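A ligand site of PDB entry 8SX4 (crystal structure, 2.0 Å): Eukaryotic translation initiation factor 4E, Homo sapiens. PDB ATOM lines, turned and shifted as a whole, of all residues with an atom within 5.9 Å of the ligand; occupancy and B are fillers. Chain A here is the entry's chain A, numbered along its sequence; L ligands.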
ATOM      1  N   TRP A  20     -12.922 -12.441 -21.923  1.00  0.00           N
ATOM      2  CA  TRP A  20     -14.225 -12.038 -21.432  1.00  0.00           C
ATOM      3  C   TRP A  20     -14.991 -11.303 -22.514  1.00  0.00           C
ATOM      4  O   TRP A  20     -14.383 -10.696 -23.399  1.00  0.00           O
ATOM      5  CB  TRP A  20     -14.072 -11.064 -20.250  1.00  0.00           C
ATOM      6  CG  TRP A  20     -13.488 -11.631 -19.011  1.00  0.00           C
ATOM      7  CD1 TRP A  20     -12.162 -11.889 -18.768  1.00  0.00           C
ATOM      8  CD2 TRP A  20     -14.173 -11.839 -17.766  1.00  0.00           C
ATOM      9  NE1 TRP A  20     -11.995 -12.318 -17.484  1.00  0.00           N
ATOM     10  CE2 TRP A  20     -13.218 -12.289 -16.837  1.00  0.00           C
ATOM     11  CE3 TRP A  20     -15.506 -11.722 -17.355  1.00  0.00           C
ATOM     12  CZ2 TRP A  20     -13.546 -12.629 -15.520  1.00  0.00           C
ATOM     13  CZ3 TRP A  20     -15.845 -12.056 -16.046  1.00  0.00           C
ATOM     14  CH2 TRP A  20     -14.866 -12.510 -15.154  1.00  0.00           C
ATOM     15  N   PHE A  21     -16.323 -11.289 -22.408  1.00  0.00           N
ATOM     16  CA  PHE A  21     -17.132 -10.507 -23.313  1.00  0.00           C
ATOM     17  C   PHE A  21     -18.248  -9.785 -22.539  1.00  0.00           C
ATOM     18  O   PHE A  21     -18.559 -10.122 -21.381  1.00  0.00           O
ATOM     19  CB  PHE A  21     -17.622 -11.311 -24.528  1.00  0.00           C
ATOM     20  CG  PHE A  21     -18.955 -12.005 -24.431  1.00  0.00           C
ATOM     21  CD1 PHE A  21     -19.049 -13.284 -23.904  1.00  0.00           C
ATOM     22  CD2 PHE A  21     -20.097 -11.447 -24.969  1.00  0.00           C
ATOM     23  CE1 PHE A  21     -20.262 -13.958 -23.886  1.00  0.00           C
ATOM     24  CE2 PHE A  21     -21.314 -12.117 -24.929  1.00  0.00           C
ATOM     25  CZ  PHE A  21     -21.396 -13.353 -24.361  1.00  0.00           C
ATOM     26  N   PHE A  22     -18.762  -8.716 -23.127  1.00  0.00           N
ATOM     27  CA  PHE A  22     -19.811  -7.941 -22.521  1.00  0.00           C
ATOM     28  C   PHE A  22     -21.026  -7.999 -23.437  1.00  0.00           C
ATOM     29  O   PHE A  22     -20.977  -7.445 -24.530  1.00  0.00           O
ATOM     30  CB  PHE A  22     -19.341  -6.481 -22.305  1.00  0.00           C
ATOM     31  CG  PHE A  22     -20.332  -5.634 -21.544  1.00  0.00           C
ATOM     32  CD1 PHE A  22     -21.310  -4.925 -22.226  1.00  0.00           C
ATOM     33  CD2 PHE A  22     -20.284  -5.546 -20.170  1.00  0.00           C
ATOM     34  CE1 PHE A  22     -22.233  -4.155 -21.538  1.00  0.00           C
ATOM     35  CE2 PHE A  22     -21.223  -4.779 -19.488  1.00  0.00           C
ATOM     36  CZ  PHE A  22     -22.178  -4.071 -20.166  1.00  0.00           C
ATOM     37  N   TRP A  30     -24.676  -3.124 -14.977  1.00  0.00           N
ATOM     38  CA  TRP A  30     -23.441  -3.338 -15.720  1.00  0.00           C
ATOM     39  C   TRP A  30     -22.741  -4.697 -15.533  1.00  0.00           C
ATOM     40  O   TRP A  30     -22.596  -5.408 -16.514  1.00  0.00           O
ATOM     41  CB  TRP A  30     -22.420  -2.209 -15.480  1.00  0.00           C
ATOM     42  CG  TRP A  30     -21.328  -2.219 -16.516  1.00  0.00           C
ATOM     43  CD1 TRP A  30     -21.397  -1.693 -17.768  1.00  0.00           C
ATOM     44  CD2 TRP A  30     -20.059  -2.879 -16.427  1.00  0.00           C
ATOM     45  NE1 TRP A  30     -20.241  -1.986 -18.465  1.00  0.00           N
ATOM     46  CE2 TRP A  30     -19.379  -2.656 -17.639  1.00  0.00           C
ATOM     47  CE3 TRP A  30     -19.400  -3.584 -15.410  1.00  0.00           C
ATOM     48  CZ2 TRP A  30     -18.118  -3.201 -17.902  1.00  0.00           C
ATOM     49  CZ3 TRP A  30     -18.131  -4.064 -15.650  1.00  0.00           C
ATOM     50  CH2 TRP A  30     -17.499  -3.873 -16.884  1.00  0.00           C
ATOM     51  N   GLN A  31     -22.322  -5.072 -14.305  1.00  0.00           N
ATOM     52  CA  GLN A  31     -21.575  -6.309 -14.112  1.00  0.00           C
ATOM     53  C   GLN A  31     -22.324  -7.570 -14.467  1.00  0.00           C
ATOM     54  O   GLN A  31     -21.686  -8.578 -14.760  1.00  0.00           O
ATOM     55  CB  GLN A  31     -21.012  -6.440 -12.689  1.00  0.00           C
ATOM     56  CG  GLN A  31     -20.164  -5.269 -12.220  1.00  0.00           C
ATOM     57  CD  GLN A  31     -19.692  -5.499 -10.791  1.00  0.00           C
ATOM     58  OE1 GLN A  31     -19.505  -6.640 -10.344  1.00  0.00           O
ATOM     59  NE2 GLN A  31     -19.505  -4.417 -10.054  1.00  0.00           N
ATOM     60  N   LEU A  34     -21.230  -9.069 -17.865  1.00  0.00           N
ATOM     61  CA  LEU A  34     -19.890  -9.621 -18.085  1.00  0.00           C
ATOM     62  C   LEU A  34     -19.953 -11.133 -18.176  1.00  0.00           C
ATOM     63  O   LEU A  34     -20.659 -11.775 -17.403  1.00  0.00           O
ATOM     64  CB  LEU A  34     -18.969  -9.269 -16.907  1.00  0.00           C
ATOM     65  CG  LEU A  34     -18.391  -7.859 -16.884  1.00  0.00           C
ATOM     66  CD1 LEU A  34     -17.492  -7.675 -15.658  1.00  0.00           C
ATOM     67  CD2 LEU A  34     -17.573  -7.577 -18.147  1.00  0.00           C
ATOM     68  N   ASP A  64     -18.626  -5.900 -26.895  1.00  0.00           N
ATOM     69  CA  ASP A  64     -17.234  -5.725 -26.479  1.00  0.00           C
ATOM     70  C   ASP A  64     -16.550  -6.979 -25.922  1.00  0.00           C
ATOM     71  O   ASP A  64     -17.212  -7.881 -25.401  1.00  0.00           O
ATOM     72  CB  ASP A  64     -17.161  -4.572 -25.484  1.00  0.00           C
ATOM     73  CG  ASP A  64     -17.809  -3.274 -25.955  1.00  0.00           C
ATOM     74  OD1 ASP A  64     -18.110  -3.165 -27.153  1.00  0.00           O
ATOM     75  OD2 ASP A  64     -17.986  -2.362 -25.119  1.00  0.00           O
ATOM     76  N   TYR A  65     -15.217  -7.028 -26.040  1.00  0.00           N
ATOM     77  CA  TYR A  65     -14.418  -8.158 -25.575  1.00  0.00           C
ATOM     78  C   TYR A  65     -13.191  -7.648 -24.771  1.00  0.00           C
ATOM     79  O   TYR A  65     -12.772  -6.483 -24.909  1.00  0.00           O
ATOM     80  CB  TYR A  65     -13.856  -8.965 -26.776  1.00  0.00           C
ATOM     81  CG  TYR A  65     -14.824  -9.934 -27.412  1.00  0.00           C
ATOM     82  CD1 TYR A  65     -15.708  -9.516 -28.401  1.00  0.00           C
ATOM     83  CD2 TYR A  65     -14.741 -11.295 -27.148  1.00  0.00           C
ATOM     84  CE1 TYR A  65     -16.566 -10.419 -29.028  1.00  0.00           C
ATOM     85  CE2 TYR A  65     -15.601 -12.207 -27.765  1.00  0.00           C
ATOM     86  CZ  TYR A  65     -16.513 -11.759 -28.704  1.00  0.00           C
ATOM     87  OH  TYR A  65     -17.347 -12.653 -29.347  1.00  0.00           O
ATOM     88  N   SER A  66     -12.584  -8.546 -23.979  1.00  0.00           N
ATOM     89  CA  SER A  66     -11.377  -8.202 -23.251  1.00  0.00           C
ATOM     90  C   SER A  66     -10.531  -9.438 -22.959  1.00  0.00           C
ATOM     91  O   SER A  66     -11.041 -10.565 -22.972  1.00  0.00           O
ATOM     92  CB  SER A  66     -11.691  -7.433 -21.968  1.00  0.00           C
ATOM     93  OG  SER A  66     -12.505  -8.192 -21.094  1.00  0.00           O
ATOM     94  N   PHE A  68      -7.808 -10.497 -20.049  1.00  0.00           N
ATOM     95  CA  PHE A  68      -7.178 -10.050 -18.795  1.00  0.00           C
ATOM     96  C   PHE A  68      -6.394 -11.185 -18.203  1.00  0.00           C
ATOM     97  O   PHE A  68      -6.740 -12.360 -18.424  1.00  0.00           O
ATOM     98  CB  PHE A  68      -8.219  -9.535 -17.794  1.00  0.00           C
ATOM     99  CG  PHE A  68      -8.479  -8.059 -17.946  1.00  0.00           C
ATOM    100  CD1 PHE A  68      -9.186  -7.573 -19.036  1.00  0.00           C
ATOM    101  CD2 PHE A  68      -7.965  -7.152 -17.030  1.00  0.00           C
ATOM    102  CE1 PHE A  68      -9.381  -6.202 -19.210  1.00  0.00           C
ATOM    103  CE2 PHE A  68      -8.184  -5.790 -17.189  1.00  0.00           C
ATOM    104  CZ  PHE A  68      -8.892  -5.326 -18.279  1.00  0.00           C
ATOM    105  N   PRO A  74     -12.322  -7.923 -15.704  1.00  0.00           N
ATOM    106  CA  PRO A  74     -12.160  -6.741 -16.562  1.00  0.00           C
ATOM    107  C   PRO A  74     -13.058  -5.593 -16.126  1.00  0.00           C
ATOM    108  O   PRO A  74     -13.982  -5.212 -16.839  1.00  0.00           O
ATOM    109  CB  PRO A  74     -12.572  -7.282 -17.946  1.00  0.00           C
ATOM    110  CG  PRO A  74     -13.606  -8.304 -17.630  1.00  0.00           C
ATOM    111  CD  PRO A  74     -13.096  -8.968 -16.380  1.00  0.00           C
ATOM    112  N   MET A  75     -12.829  -5.102 -14.917  1.00  0.00           N
ATOM    113  CA  MET A  75     -13.628  -4.000 -14.373  1.00  0.00           C
ATOM    114  C   MET A  75     -12.844  -3.134 -13.421  1.00  0.00           C
ATOM    115  O   MET A  75     -11.952  -3.625 -12.727  1.00  0.00           O
ATOM    116  CB  MET A  75     -14.927  -4.523 -13.729  1.00  0.00           C
ATOM    117  CG  MET A  75     -14.719  -5.306 -12.474  1.00  0.00           C
ATOM    118  SD  MET A  75     -16.287  -6.128 -11.978  1.00  0.00           S
ATOM    119  CE  MET A  75     -15.691  -7.066 -10.578  1.00  0.00           C
ATOM    120  N   TRP A  76     -13.176  -1.834 -13.392  1.00  0.00           N
ATOM    121  CA  TRP A  76     -12.530  -0.842 -12.513  1.00  0.00           C
ATOM    122  C   TRP A  76     -12.513  -1.312 -11.049  1.00  0.00           C
ATOM    123  O   TRP A  76     -11.525  -1.113 -10.349  1.00  0.00           O
ATOM    124  CB  TRP A  76     -13.292   0.493 -12.573  1.00  0.00           C
ATOM    125  CG  TRP A  76     -13.454   1.072 -13.933  1.00  0.00           C
ATOM    126  CD1 TRP A  76     -12.561   1.023 -14.965  1.00  0.00           C
ATOM    127  CD2 TRP A  76     -14.534   1.911 -14.387  1.00  0.00           C
ATOM    128  NE1 TRP A  76     -13.025   1.743 -16.038  1.00  0.00           N
ATOM    129  CE2 TRP A  76     -14.253   2.275 -15.712  1.00  0.00           C
ATOM    130  CE3 TRP A  76     -15.735   2.345 -13.805  1.00  0.00           C
ATOM    131  CZ2 TRP A  76     -15.096   3.089 -16.462  1.00  0.00           C
ATOM    132  CZ3 TRP A  76     -16.569   3.166 -14.536  1.00  0.00           C
ATOM    133  CH2 TRP A  76     -16.253   3.524 -15.849  1.00  0.00           C
ATOM    134  N   GLU A  77     -13.598  -1.969 -10.639  1.00  0.00           N
ATOM    135  CA  GLU A  77     -13.874  -2.518  -9.306  1.00  0.00           C
ATOM    136  C   GLU A  77     -12.884  -3.498  -8.796  1.00  0.00           C
ATOM    137  O   GLU A  77     -12.713  -3.592  -7.586  1.00  0.00           O
ATOM    138  CB  GLU A  77     -15.257  -3.166  -9.267  1.00  0.00           C
ATOM    139  CG  GLU A  77     -16.354  -2.130  -9.335  1.00  0.00           C
ATOM    140  CD  GLU A  77     -16.866  -1.818 -10.729  1.00  0.00           C
ATOM    141  OE1 GLU A  77     -16.164  -2.148 -11.710  1.00  0.00           O
ATOM    142  OE2 GLU A  77     -17.959  -1.220 -10.823  1.00  0.00           O
ATOM    143  N   ARG A  86      -5.864   3.306 -18.109  1.00  0.00           N
ATOM    144  CA  ARG A  86      -5.721   2.696 -19.435  1.00  0.00           C
ATOM    145  C   ARG A  86      -5.125   3.642 -20.463  1.00  0.00           C
ATOM    146  O   ARG A  86      -5.347   4.851 -20.403  1.00  0.00           O
ATOM    147  CB  ARG A  86      -7.099   2.246 -19.922  1.00  0.00           C
ATOM    148  CG  ARG A  86      -8.070   3.429 -20.002  1.00  0.00           C
ATOM    149  CD  ARG A  86      -9.324   3.110 -20.737  1.00  0.00           C
ATOM    150  NE  ARG A  86     -10.162   4.308 -20.879  1.00  0.00           N
ATOM    151  CZ  ARG A  86     -11.387   4.308 -21.388  1.00  0.00           C
ATOM    152  NH1 ARG A  86     -11.928   3.189 -21.836  1.00  0.00           N
ATOM    153  NH2 ARG A  86     -12.082   5.447 -21.444  1.00  0.00           N
ATOM    154  N   VAL A 127      -9.000  -4.075 -23.550  1.00  0.00           N
ATOM    155  CA  VAL A 127     -10.447  -4.006 -23.846  1.00  0.00           C
ATOM    156  C   VAL A 127     -10.677  -3.426 -25.241  1.00  0.00           C
ATOM    157  O   VAL A 127     -10.037  -2.432 -25.597  1.00  0.00           O
ATOM    158  CB  VAL A 127     -11.213  -3.167 -22.769  1.00  0.00           C
ATOM    159  CG1 VAL A 127     -12.699  -3.013 -23.123  1.00  0.00           C
ATOM    160  CG2 VAL A 127     -11.047  -3.758 -21.370  1.00  0.00           C
ATOM    161  N   VAL A 128     -11.545  -4.052 -26.046  1.00  0.00           N
ATOM    162  CA  VAL A 128     -11.913  -3.492 -27.337  1.00  0.00           C
ATOM    163  C   VAL A 128     -13.425  -3.145 -27.283  1.00  0.00           C
ATOM    164  O   VAL A 128     -14.247  -3.995 -26.937  1.00  0.00           O
ATOM    165  CB  VAL A 128     -11.537  -4.369 -28.559  1.00  0.00           C
ATOM    166  CG1 VAL A 128     -11.884  -5.842 -28.343  1.00  0.00           C
ATOM    167  CG2 VAL A 128     -12.208  -3.849 -29.841  1.00  0.00           C
ATOM    168  N   ASN A 129     -13.775  -1.879 -27.549  1.00  0.00           N
ATOM    169  CA  ASN A 129     -15.171  -1.463 -27.560  1.00  0.00           C
ATOM    170  C   ASN A 129     -15.655  -1.330 -29.001  1.00  0.00           C
ATOM    171  O   ASN A 129     -15.136  -0.492 -29.739  1.00  0.00           O
ATOM    172  CB  ASN A 129     -15.393  -0.156 -26.794  1.00  0.00           C
ATOM    173  CG  ASN A 129     -14.829  -0.152 -25.384  1.00  0.00           C
ATOM    174  OD1 ASN A 129     -13.864   0.555 -25.082  1.00  0.00           O
ATOM    175  ND2 ASN A 129     -15.394  -0.954 -24.500  1.00  0.00           N
ATOM    176  N   ARG A 131     -18.144   0.042 -31.353  1.00  0.00           N
ATOM    177  CA  ARG A 131     -19.220   1.038 -31.346  1.00  0.00           C
ATOM    178  C   ARG A 131     -19.568   1.534 -32.738  1.00  0.00           C
ATOM    179  O   ARG A 131     -18.678   1.824 -33.534  1.00  0.00           O
ATOM    180  CB  ARG A 131     -18.811   2.258 -30.510  1.00  0.00           C
ATOM    181  CG  ARG A 131     -18.524   1.972 -29.040  1.00  0.00           C
ATOM    182  CD  ARG A 131     -19.784   2.003 -28.188  1.00  0.00           C
ATOM    183  NE  ARG A 131     -19.446   2.039 -26.764  1.00  0.00           N
ATOM    184  CZ  ARG A 131     -19.240   0.956 -26.019  1.00  0.00           C
ATOM    185  NH1 ARG A 131     -19.326  -0.257 -26.551  1.00  0.00           N
ATOM    186  NH2 ARG A 131     -18.929   1.076 -24.738  1.00  0.00           N
ATOM    187  N   LYS A 136     -12.901   1.579 -30.026  1.00  0.00           N
ATOM    188  CA  LYS A 136     -11.841   1.971 -29.116  1.00  0.00           C
ATOM    189  C   LYS A 136     -11.069   0.731 -28.652  1.00  0.00           C
ATOM    190  O   LYS A 136     -11.642  -0.354 -28.554  1.00  0.00           O
ATOM    191  CB  LYS A 136     -12.416   2.706 -27.896  1.00  0.00           C
ATOM    192  CG  LYS A 136     -13.126   4.029 -28.175  1.00  0.00           C
ATOM    193  CD  LYS A 136     -13.821   4.502 -26.899  1.00  0.00           C
ATOM    194  CE  LYS A 136     -14.288   5.929 -26.932  1.00  0.00           C
ATOM    195  NZ  LYS A 136     -14.366   6.497 -25.542  1.00  0.00           N
ATOM    196  N   TRP A 140      -5.002  -1.797 -20.141  1.00  0.00           N
ATOM    197  CA  TRP A 140      -5.230  -1.478 -18.739  1.00  0.00           C
ATOM    198  C   TRP A 140      -4.020  -1.823 -17.917  1.00  0.00           C
ATOM    199  O   TRP A 140      -3.422  -2.892 -18.101  1.00  0.00           O
ATOM    200  CB  TRP A 140      -6.457  -2.267 -18.230  1.00  0.00           C
ATOM    201  CG  TRP A 140      -7.794  -1.721 -18.680  1.00  0.00           C
ATOM    202  CD1 TRP A 140      -8.108  -1.220 -19.915  1.00  0.00           C
ATOM    203  CD2 TRP A 140      -9.021  -1.763 -17.944  1.00  0.00           C
ATOM    204  NE1 TRP A 140      -9.437  -0.842 -19.944  1.00  0.00           N
ATOM    205  CE2 TRP A 140     -10.025  -1.186 -18.751  1.00  0.00           C
ATOM    206  CE3 TRP A 140      -9.369  -2.243 -16.671  1.00  0.00           C
ATOM    207  CZ2 TRP A 140     -11.352  -1.084 -18.332  1.00  0.00           C
ATOM    208  CZ3 TRP A 140     -10.682  -2.114 -16.255  1.00  0.00           C
ATOM    209  CH2 TRP A 140     -11.660  -1.577 -17.101  1.00  0.00           C
HETATM  210  C1  LIG L   1     -19.491   1.935 -17.940  1.00  0.00           C
HETATM  211  C2  LIG L   1     -20.162   1.554 -19.221  1.00  0.00           C
HETATM  212  C3  LIG L   1     -20.095   2.195 -20.386  1.00  0.00           C
HETATM  213  N1  LIG L   1     -19.067  -0.255 -13.159  1.00  0.00           N
HETATM  214  C4  LIG L   1     -19.295   3.438 -20.673  1.00  0.00           C
HETATM  215  C5  LIG L   1     -17.327   0.811 -18.453  1.00  0.00           C
HETATM  216  N2  LIG L   1     -18.903   0.450 -15.353  1.00  0.00           N
HETATM  217  O1  LIG L   1     -15.252  -1.467 -15.353  1.00  0.00           O
HETATM  218  C6  LIG L   1     -18.102   0.425 -16.434  1.00  0.00           C
HETATM  219  C7  LIG L   1     -16.899  -0.192 -16.542  1.00  0.00           C
HETATM  220  N3  LIG L   1     -17.190  -0.851 -14.346  1.00  0.00           N
HETATM  221  C8  LIG L   1     -18.396  -0.204 -14.307  1.00  0.00           C
HETATM  222  C9  LIG L   1     -16.332  -0.897 -15.431  1.00  0.00           C
HETATM  223 CL1  LIG L   1     -15.463  -7.365 -21.487  1.00  0.00          CL
HETATM  224  C10 LIG L   1     -15.574  -5.642 -21.219  1.00  0.00           C
HETATM  225  C11 LIG L   1     -15.040  -5.115 -20.051  1.00  0.00           C
HETATM  226  C12 LIG L   1     -16.166  -4.844 -22.185  1.00  0.00           C
HETATM  227  C13 LIG L   1     -16.225  -3.474 -21.990  1.00  0.00           C
HETATM  228  C14 LIG L   1     -15.717  -2.933 -20.815  1.00  0.00           C
HETATM  229  C15 LIG L   1     -15.111  -3.737 -19.832  1.00  0.00           C
HETATM  230  C16 LIG L   1     -14.760  -2.866 -18.744  1.00  0.00           C
HETATM  231  N4  LIG L   1     -15.750  -1.636 -20.332  1.00  0.00           N
HETATM  232  C17 LIG L   1     -15.179  -1.557 -19.095  1.00  0.00           C
HETATM  233  C18 LIG L   1     -15.101  -0.277 -18.341  1.00  0.00           C
HETATM  234  N5  LIG L   1     -16.429   0.049 -17.827  1.00  0.00           N
HETATM  235  N6  LIG L   1     -18.347   1.050 -17.627  1.00  0.00           N
HETATM  236  P1  LIG L   1     -18.422   3.382 -22.247  1.00  0.00           P
HETATM  237  O2  LIG L   1     -19.333   3.701 -23.390  1.00  0.00           O
HETATM  238  O3  LIG L   1     -17.254   4.397 -22.141  1.00  0.00           O
HETATM  239  O4  LIG L   1     -17.785   1.967 -22.347  1.00  0.00           O
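The side-chain sulfur (SD) of Met 75 sits close to the side-chain amide oxygen (OE1) of Gln 31, at 3.6 Å.
The side-chain amide nitrogen (ND2) of Asn 129 lies within hydrogen-bond range of the side-chain carboxylate (OD2) of Asp 64, at 3.0 Å.
NH1 of Arg 131 lies within salt-bridge range of OD2 of Asp 64 (2.9 Å).
N of Trp 20 is in hydrogen-bond range of O of Ser 66, at 2.9 Å.
N of Asn 129 sits at hydrogen-bond distance from O of Lys 136 (2.8 Å).
The backbone carbonyl oxygen (O) of Asp 64 sits at hydrogen-bond distance from the backbone NH (N) of Phe 22, at 2.9 Å.
NH2 of Arg 131 lies within salt-bridge range of O4 of the ligand (2.8 Å).
A nitrogen (N1) of the ligand sits at hydrogen-bond distance from the side-chain carboxylate (OE2) of Glu 77 (2.8 Å).
The backbone NH of Trp 76 sits at hydrogen-bond distance from an oxygen (O1) of the ligand, at 2.9 Å.
Trp 20 touches the ligand (O to CL1, 3.99 Å).
C of Phe 21 touches CL1 of the ligand, at 3.8 Å.
Phe 22 touches the ligand (CB to C12, 3.6 Å).
Trp 30 touches the ligand.
Leu 34 touches the ligand.
Asp 64 touches the ligand (CB to C12, 3.5 Å).
Ser 66 touches the ligand.
Pro 74 touches the ligand (O to C16, 3.1 Å).
Met 75 touches the ligand.
CG1 of Val 127 touches C13 of the ligand (3.7 Å).
Asn 129 touches the ligand (ND2 to C13, 3.7 Å).
CH2 of Trp 140 touches C16 of the ligand, at 3.7 Å.
Hydrophobic or aromatic side chains within 4 Å of the ligand: Phe 22, Trp 30, Leu 34, Pro 74, Met 75, Trp 76, Val 127 and Trp 140.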
